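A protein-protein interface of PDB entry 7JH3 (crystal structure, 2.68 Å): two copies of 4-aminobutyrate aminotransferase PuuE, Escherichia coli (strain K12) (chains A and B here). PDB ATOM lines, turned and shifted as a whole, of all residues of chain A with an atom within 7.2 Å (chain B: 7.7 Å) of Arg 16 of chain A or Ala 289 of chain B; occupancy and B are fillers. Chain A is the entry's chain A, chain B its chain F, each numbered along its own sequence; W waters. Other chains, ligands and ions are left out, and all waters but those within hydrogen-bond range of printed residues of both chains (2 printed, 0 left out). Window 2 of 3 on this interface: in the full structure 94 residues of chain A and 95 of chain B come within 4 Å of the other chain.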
ATOM      1  N   ARG A  10      14.028  20.790 -37.792  1.00  0.00           N
ATOM      2  CA  ARG A  10      14.285  19.519 -37.124  1.00  0.00           C
ATOM      3  C   ARG A  10      13.841  19.579 -35.668  1.00  0.00           C
ATOM      4  O   ARG A  10      13.088  18.724 -35.194  1.00  0.00           O
ATOM      5  CB  ARG A  10      15.769  19.159 -37.222  1.00  0.00           C
ATOM      6  CG  ARG A  10      16.099  17.795 -36.627  1.00  0.00           C
ATOM      7  CD  ARG A  10      17.595  17.500 -36.650  1.00  0.00           C
ATOM      8  NE  ARG A  10      18.360  18.368 -35.757  1.00  0.00           N
ATOM      9  CZ  ARG A  10      18.384  18.246 -34.433  1.00  0.00           C
ATOM     10  NH1 ARG A  10      17.672  17.297 -33.836  1.00  0.00           N
ATOM     11  NH2 ARG A  10      19.115  19.083 -33.705  1.00  0.00           N
ATOM     12  N   LEU A  11      14.300  20.607 -34.947  1.00  0.00           N
ATOM     13  CA  LEU A  11      13.915  20.761 -33.549  1.00  0.00           C
ATOM     14  C   LEU A  11      12.402  20.852 -33.385  1.00  0.00           C
ATOM     15  O   LEU A  11      11.860  20.399 -32.371  1.00  0.00           O
ATOM     16  CB  LEU A  11      14.594  21.992 -32.952  1.00  0.00           C
ATOM     17  CG  LEU A  11      16.117  21.900 -32.820  1.00  0.00           C
ATOM     18  CD1 LEU A  11      16.703  23.243 -32.417  1.00  0.00           C
ATOM     19  CD2 LEU A  11      16.501  20.826 -31.816  1.00  0.00           C
ATOM     20  N   THR A  14      10.700  16.898 -34.615  1.00  0.00           N
ATOM     21  CA  THR A  14      11.175  15.663 -34.018  1.00  0.00           C
ATOM     22  C   THR A  14      11.410  15.842 -32.523  1.00  0.00           C
ATOM     23  O   THR A  14      11.626  16.963 -32.049  1.00  0.00           O
ATOM     24  CB  THR A  14      12.472  15.198 -34.698  1.00  0.00           C
ATOM     25  OG1 THR A  14      13.563  16.034 -34.290  1.00  0.00           O
ATOM     26  CG2 THR A  14      12.327  15.266 -36.209  1.00  0.00           C
ATOM     27  N   PRO A  15      11.368  14.759 -31.747  1.00  0.00           N
ATOM     28  CA  PRO A  15      11.558  14.891 -30.299  1.00  0.00           C
ATOM     29  C   PRO A  15      12.978  15.311 -29.953  1.00  0.00           C
ATOM     30  O   PRO A  15      13.928  15.058 -30.697  1.00  0.00           O
ATOM     31  CB  PRO A  15      11.254  13.482 -29.767  1.00  0.00           C
ATOM     32  CG  PRO A  15      10.523  12.783 -30.871  1.00  0.00           C
ATOM     33  CD  PRO A  15      11.062  13.371 -32.137  1.00  0.00           C
ATOM     34  N   ARG A  16      13.114  15.968 -28.798  1.00  0.00           N
ATOM     35  CA  ARG A  16      14.438  16.335 -28.306  1.00  0.00           C
ATOM     36  C   ARG A  16      15.281  15.113 -27.965  1.00  0.00           C
ATOM     37  O   ARG A  16      16.514  15.206 -27.968  1.00  0.00           O
ATOM     38  CB  ARG A  16      14.314  17.239 -27.077  1.00  0.00           C
ATOM     39  CG  ARG A  16      13.638  16.562 -25.886  1.00  0.00           C
ATOM     40  CD  ARG A  16      13.240  17.552 -24.798  1.00  0.00           C
ATOM     41  NE  ARG A  16      14.261  17.703 -23.765  1.00  0.00           N
ATOM     42  CZ  ARG A  16      14.274  17.030 -22.618  1.00  0.00           C
ATOM     43  NH1 ARG A  16      13.322  16.150 -22.351  1.00  0.00           N
ATOM     44  NH2 ARG A  16      15.242  17.238 -21.736  1.00  0.00           N
ATOM     45  N   GLY A  17      14.645  13.970 -27.679  1.00  0.00           N
ATOM     46  CA  GLY A  17      15.380  12.794 -27.241  1.00  0.00           C
ATOM     47  C   GLY A  17      16.246  12.178 -28.320  1.00  0.00           C
ATOM     48  O   GLY A  17      17.292  11.594 -28.023  1.00  0.00           O
ATOM     49  N   VAL A  18      15.826  12.279 -29.576  1.00  0.00           N
ATOM     50  CA  VAL A  18      16.684  11.883 -30.685  1.00  0.00           C
ATOM     51  C   VAL A  18      17.752  12.960 -30.813  1.00  0.00           C
ATOM     52  O   VAL A  18      17.534  13.997 -31.451  1.00  0.00           O
ATOM     53  CB  VAL A  18      15.876  11.704 -31.982  1.00  0.00           C
ATOM     54  CG1 VAL A  18      16.793  11.305 -33.129  1.00  0.00           C
ATOM     55  CG2 VAL A  18      14.782  10.667 -31.779  1.00  0.00           C
ATOM     56  N   GLY A  19      18.903  12.736 -30.182  1.00  0.00           N
ATOM     57  CA  GLY A  19      19.963  13.734 -30.189  1.00  0.00           C
ATOM     58  C   GLY A  19      20.740  13.696 -31.497  1.00  0.00           C
ATOM     59  O   GLY A  19      20.983  12.636 -32.075  1.00  0.00           O
ATOM     60  N   VAL A  20      21.135  14.881 -31.959  1.00  0.00           N
ATOM     61  CA  VAL A  20      21.857  15.044 -33.215  1.00  0.00           C
ATOM     62  C   VAL A  20      23.143  15.807 -32.939  1.00  0.00           C
ATOM     63  O   VAL A  20      23.120  16.864 -32.298  1.00  0.00           O
ATOM     64  CB  VAL A  20      21.009  15.775 -34.272  1.00  0.00           C
ATOM     65  CG1 VAL A  20      21.863  16.141 -35.463  1.00  0.00           C
ATOM     66  CG2 VAL A  20      19.832  14.904 -34.696  1.00  0.00           C
ATOM     67  N   PRO A 153      23.558   8.427 -21.246  1.00  0.00           N
ATOM     68  CA  PRO A 153      22.155   8.832 -21.148  1.00  0.00           C
ATOM     69  C   PRO A 153      21.163   7.748 -21.579  1.00  0.00           C
ATOM     70  O   PRO A 153      19.967   8.031 -21.697  1.00  0.00           O
ATOM     71  CB  PRO A 153      22.092  10.013 -22.110  1.00  0.00           C
ATOM     72  CG  PRO A 153      23.040   9.600 -23.220  1.00  0.00           C
ATOM     73  CD  PRO A 153      24.109   8.724 -22.581  1.00  0.00           C
ATOM     74  N   ILE A 156      18.418   6.594 -18.761  1.00  0.00           N
ATOM     75  CA  ILE A 156      17.760   7.585 -17.875  1.00  0.00           C
ATOM     76  C   ILE A 156      16.253   7.578 -18.131  1.00  0.00           C
ATOM     77  O   ILE A 156      15.847   7.802 -19.250  1.00  0.00           O
ATOM     78  CB  ILE A 156      18.363   8.963 -18.162  1.00  0.00           C
ATOM     79  CG1 ILE A 156      19.887   8.936 -18.181  1.00  0.00           C
ATOM     80  CG2 ILE A 156      17.815  10.008 -17.225  1.00  0.00           C
ATOM     81  CD1 ILE A 156      20.528   8.989 -16.846  1.00  0.00           C
ATOM     82  N   PHE A 158      14.031   5.163 -18.122  1.00  0.00           N
ATOM     83  CA  PHE A 158      13.395   4.060 -18.874  1.00  0.00           C
ATOM     84  C   PHE A 158      13.231   2.816 -18.008  1.00  0.00           C
ATOM     85  O   PHE A 158      12.727   1.834 -18.498  1.00  0.00           O
ATOM     86  CB  PHE A 158      14.194   3.784 -20.142  1.00  0.00           C
ATOM     87  CG  PHE A 158      14.376   4.981 -21.029  1.00  0.00           C
ATOM     88  CD1 PHE A 158      13.285   5.700 -21.472  1.00  0.00           C
ATOM     89  CD2 PHE A 158      15.630   5.384 -21.425  1.00  0.00           C
ATOM     90  CE1 PHE A 158      13.442   6.793 -22.295  1.00  0.00           C
ATOM     91  CE2 PHE A 158      15.784   6.486 -22.235  1.00  0.00           C
ATOM     92  CZ  PHE A 158      14.692   7.179 -22.673  1.00  0.00           C
ATOM     93  N   LYS B 103       4.826  15.391 -32.733  1.00  0.00           N
ATOM     94  CA  LYS B 103       6.212  15.205 -33.134  1.00  0.00           C
ATOM     95  C   LYS B 103       6.412  13.741 -33.505  1.00  0.00           C
ATOM     96  O   LYS B 103       5.732  12.850 -32.980  1.00  0.00           O
ATOM     97  CB  LYS B 103       7.199  15.612 -32.032  1.00  0.00           C
ATOM     98  CG  LYS B 103       7.330  17.111 -31.844  1.00  0.00           C
ATOM     99  CD  LYS B 103       8.478  17.448 -30.907  1.00  0.00           C
ATOM    100  CE  LYS B 103       8.651  18.957 -30.766  1.00  0.00           C
ATOM    101  NZ  LYS B 103       9.899  19.322 -30.035  1.00  0.00           N
ATOM    102  N   ALA B 123       9.206   7.572 -19.474  1.00  0.00           N
ATOM    103  CA  ALA B 123       9.916   8.803 -19.140  1.00  0.00           C
ATOM    104  C   ALA B 123       8.944   9.930 -18.819  1.00  0.00           C
ATOM    105  O   ALA B 123       9.211  10.755 -17.937  1.00  0.00           O
ATOM    106  CB  ALA B 123      10.844   9.206 -20.285  1.00  0.00           C
ATOM    107  N   ALA B 282       3.494  16.279 -28.799  1.00  0.00           N
ATOM    108  CA  ALA B 282       4.851  16.818 -28.736  1.00  0.00           C
ATOM    109  C   ALA B 282       5.377  16.860 -27.306  1.00  0.00           C
ATOM    110  O   ALA B 282       6.530  16.493 -27.051  1.00  0.00           O
ATOM    111  CB  ALA B 282       4.892  18.211 -29.362  1.00  0.00           C
ATOM    112  N   ASN B 283       4.543  17.297 -26.358  1.00  0.00           N
ATOM    113  CA  ASN B 283       4.988  17.390 -24.970  1.00  0.00           C
ATOM    114  C   ASN B 283       5.377  16.024 -24.420  1.00  0.00           C
ATOM    115  O   ASN B 283       6.361  15.902 -23.680  1.00  0.00           O
ATOM    116  CB  ASN B 283       3.896  18.027 -24.113  1.00  0.00           C
ATOM    117  CG  ASN B 283       3.589  19.456 -24.524  1.00  0.00           C
ATOM    118  OD1 ASN B 283       4.452  20.163 -25.049  1.00  0.00           O
ATOM    119  ND2 ASN B 283       2.358  19.887 -24.283  1.00  0.00           N
ATOM    120  N   ILE B 284       4.624  14.984 -24.777  1.00  0.00           N
ATOM    121  CA  ILE B 284       4.934  13.643 -24.295  1.00  0.00           C
ATOM    122  C   ILE B 284       6.149  13.082 -25.021  1.00  0.00           C
ATOM    123  O   ILE B 284       7.022  12.457 -24.409  1.00  0.00           O
ATOM    124  CB  ILE B 284       3.708  12.727 -24.444  1.00  0.00           C
ATOM    125  CG1 ILE B 284       2.561  13.229 -23.566  1.00  0.00           C
ATOM    126  CG2 ILE B 284       4.066  11.300 -24.082  1.00  0.00           C
ATOM    127  CD1 ILE B 284       1.310  12.385 -23.661  1.00  0.00           C
ATOM    128  N   MET B 285       6.227  13.300 -26.336  1.00  0.00           N
ATOM    129  CA  MET B 285       7.385  12.846 -27.095  1.00  0.00           C
ATOM    130  C   MET B 285       8.673  13.458 -26.562  1.00  0.00           C
ATOM    131  O   MET B 285       9.723  12.804 -26.562  1.00  0.00           O
ATOM    132  CB  MET B 285       7.207  13.186 -28.574  1.00  0.00           C
ATOM    133  CG  MET B 285       6.041  12.472 -29.235  1.00  0.00           C
ATOM    134  SD  MET B 285       6.359  10.719 -29.506  1.00  0.00           S
ATOM    135  CE  MET B 285       7.452  10.786 -30.925  1.00  0.00           C
ATOM    136  N   ASP B 286       8.615  14.705 -26.090  1.00  0.00           N
ATOM    137  CA  ASP B 286       9.794  15.401 -25.587  1.00  0.00           C
ATOM    138  C   ASP B 286      10.193  14.975 -24.175  1.00  0.00           C
ATOM    139  O   ASP B 286      11.055  15.623 -23.573  1.00  0.00           O
ATOM    140  CB  ASP B 286       9.568  16.918 -25.624  1.00  0.00           C
ATOM    141  CG  ASP B 286       9.738  17.508 -27.018  1.00  0.00           C
ATOM    142  OD1 ASP B 286      10.417  16.874 -27.857  1.00  0.00           O
ATOM    143  OD2 ASP B 286       9.202  18.613 -27.272  1.00  0.00           O
ATOM    144  N   ALA B 287       9.603  13.908 -23.630  1.00  0.00           N
ATOM    145  CA  ALA B 287       9.955  13.503 -22.269  1.00  0.00           C
ATOM    146  C   ALA B 287      11.397  13.020 -22.151  1.00  0.00           C
ATOM    147  O   ALA B 287      12.102  13.479 -21.235  1.00  0.00           O
ATOM    148  CB  ALA B 287       8.963  12.453 -21.763  1.00  0.00           C
ATOM    149  N   PRO B 288      11.901  12.118 -23.001  1.00  0.00           N
ATOM    150  CA  PRO B 288      13.299  11.692 -22.852  1.00  0.00           C
ATOM    151  C   PRO B 288      14.269  12.815 -23.195  1.00  0.00           C
ATOM    152  O   PRO B 288      14.094  13.536 -24.181  1.00  0.00           O
ATOM    153  CB  PRO B 288      13.424  10.523 -23.838  1.00  0.00           C
ATOM    154  CG  PRO B 288      12.020  10.067 -24.075  1.00  0.00           C
ATOM    155  CD  PRO B 288      11.213  11.322 -24.035  1.00  0.00           C
ATOM    156  N   ALA B 289      15.297  12.957 -22.362  1.00  0.00           N
ATOM    157  CA  ALA B 289      16.335  13.946 -22.591  1.00  0.00           C
ATOM    158  C   ALA B 289      17.138  13.589 -23.841  1.00  0.00           C
ATOM    159  O   ALA B 289      17.134  12.437 -24.281  1.00  0.00           O
ATOM    160  CB  ALA B 289      17.257  14.035 -21.378  1.00  0.00           C
ATOM    161  N   PRO B 290      17.817  14.565 -24.443  1.00  0.00           N
ATOM    162  CA  PRO B 290      18.654  14.265 -25.611  1.00  0.00           C
ATOM    163  C   PRO B 290      19.652  13.154 -25.322  1.00  0.00           C
ATOM    164  O   PRO B 290      20.292  13.117 -24.267  1.00  0.00           O
ATOM    165  CB  PRO B 290      19.350  15.599 -25.893  1.00  0.00           C
ATOM    166  CG  PRO B 290      18.366  16.621 -25.426  1.00  0.00           C
ATOM    167  CD  PRO B 290      17.696  16.017 -24.214  1.00  0.00           C
ATOM    168  N   GLY B 291      19.775  12.233 -26.272  1.00  0.00           N
ATOM    169  CA  GLY B 291      20.606  11.066 -26.103  1.00  0.00           C
ATOM    170  C   GLY B 291      19.889   9.857 -25.551  1.00  0.00           C
ATOM    171  O   GLY B 291      20.523   8.810 -25.380  1.00  0.00           O
ATOM    172  N   GLY B 292      18.589   9.964 -25.271  1.00  0.00           N
ATOM    173  CA  GLY B 292      17.837   8.865 -24.699  1.00  0.00           C
ATOM    174  C   GLY B 292      17.212   7.959 -25.737  1.00  0.00           C
ATOM    175  O   GLY B 292      16.965   6.777 -25.473  1.00  0.00           O
ATOM    176  N   LEU B 293      16.953   8.500 -26.924  1.00  0.00           N
ATOM    177  CA  LEU B 293      16.348   7.755 -28.018  1.00  0.00           C
ATOM    178  C   LEU B 293      17.306   7.701 -29.201  1.00  0.00           C
ATOM    179  O   LEU B 293      18.148   8.587 -29.380  1.00  0.00           O
ATOM    180  CB  LEU B 293      15.018   8.390 -28.453  1.00  0.00           C
ATOM    181  CG  LEU B 293      14.038   8.738 -27.331  1.00  0.00           C
ATOM    182  CD1 LEU B 293      12.782   9.402 -27.890  1.00  0.00           C
ATOM    183  CD2 LEU B 293      13.687   7.499 -26.513  1.00  0.00           C
HETATM  184  O   HOH W   1      12.340  13.254 -26.577  1.00  0.00           O
HETATM  185  O   HOH W   2      10.209  22.126 -29.850  1.00  0.00           O
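The side-chain amino group of Lys 103 of chain B lies within hydrogen-bond range of the backbone carbonyl oxygen of Leu 11 of chain A, at 3.2 Å.
The guanidinium group (NH1) of Arg 16 of chain A lies within hydrogen-bond range of the backbone carbonyl oxygen (O) of Ala 287 of chain B, 3.1 Å away.
The backbone NH of Gly 291 of chain B is in hydrogen-bond range of the backbone carbonyl oxygen of Gly 17 of chain A.
The backbone carbonyl oxygen of Asp 286 of chain B is in hydrogen-bond range of the guanidinium group of Arg 16 of chain A.
The backbone carbonyl oxygen of Gly 17 of chain A sits at hydrogen-bond distance from the backbone NH of Gly 292 of chain B (3.5 Å).
The backbone NH of Leu 293 of chain B is in hydrogen-bond range of the backbone carbonyl oxygen of Gly 17 of chain A, 3.3 Å away.
The guanidinium group (NH1) of Arg 16 of chain A lies within hydrogen-bond range of the backbone carbonyl oxygen (O) of Pro 288 of chain B, at 3.3 Å.
O of Arg 10 of chain A lies within hydrogen-bond range of OG1 of Thr 14 of chain A, at 2.9 Å.
The side-chain amino group of Lys 103 of chain B is in salt-bridge range of the side-chain carboxylate of Asp 286 of chain B (2.9 Å).
O of Thr 14 of chain A touches CD of Lys 103 of chain B, 3.4 Å away.
Ala 289 of chain B touches Arg 16 of chain A.
Pro 290 of chain B touches Arg 16 of chain A (CA to O, 3.3 Å).
Pro 288 of chain B touches Gly 17 of chain A.
Ala 289 of chain B touches Gly 17 of chain A (O to CA, 3.5 Å).
Pro 290 of chain B touches Gly 17 of chain A.
O of Gly 291 of chain B touches CG of Pro 153 of chain A (3.4 Å).
Gly 292 of chain B touches Pro 153 of chain A.
Pro 288 of chain B touches Phe 158 of chain A (CB to CZ, 3.8 Å).
Gly 292 of chain B touches Phe 158 of chain A (O to CE2, 3.5 Å).
Arg 16 of chain A touches five residues of chain B.
Of chain A, only Arg 16 (3.6 Å) and Gly 17 (3.5 Å) come within 4 Å of Ala 289 of chain B.
Of the printed residues of chain A, Ala 287 of chain B touches Arg 16.
Of the printed residues of chain A, Leu 293 of chain B touches Gly 17 (3.3 Å), Val 18 (3.8 Å) and Phe 158 (3.98 Å).
Printed residues of chain B within 4 Å of Pro 15 of chain A: Met 285 (3.6 Å) and Asp 286 (3.3 Å).
Printed residues of chain B within 4 Å of Val 18 of chain A: Leu 293 (3.8 Å).
The nearest residue of chain B that does not touch Arg 16 of chain A is Gly 291 of chain B (4.7 Å).
The nearest residue of chain A that does not touch Ala 289 of chain B is Val 18 of chain A (5.5 Å).
Of the 14 printed residues of chain B, 10 touch a printed residue of chain A.
Along chain B the printed residues that touch a printed residue of chain A span positions 103 to 293.
Among the printed residues, no Asp or Glu carboxylate lies within 4 Å of a Lys or Arg side-chain nitrogen of the other chain.
No position is printed for both chains.
Water W1 lies within hydrogen-bond range of the backbone NH (N) of Gly 17 of chain A (2.7 Å), the backbone carbonyl oxygen (O) of Met 285 of chain B (2.7 Å) and the backbone carbonyl oxygen (O) of Pro 288 of chain B (3.0 Å).
Water W2 bridges NZ of Lys 103 of chain B and O of Leu 11 of chain A.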
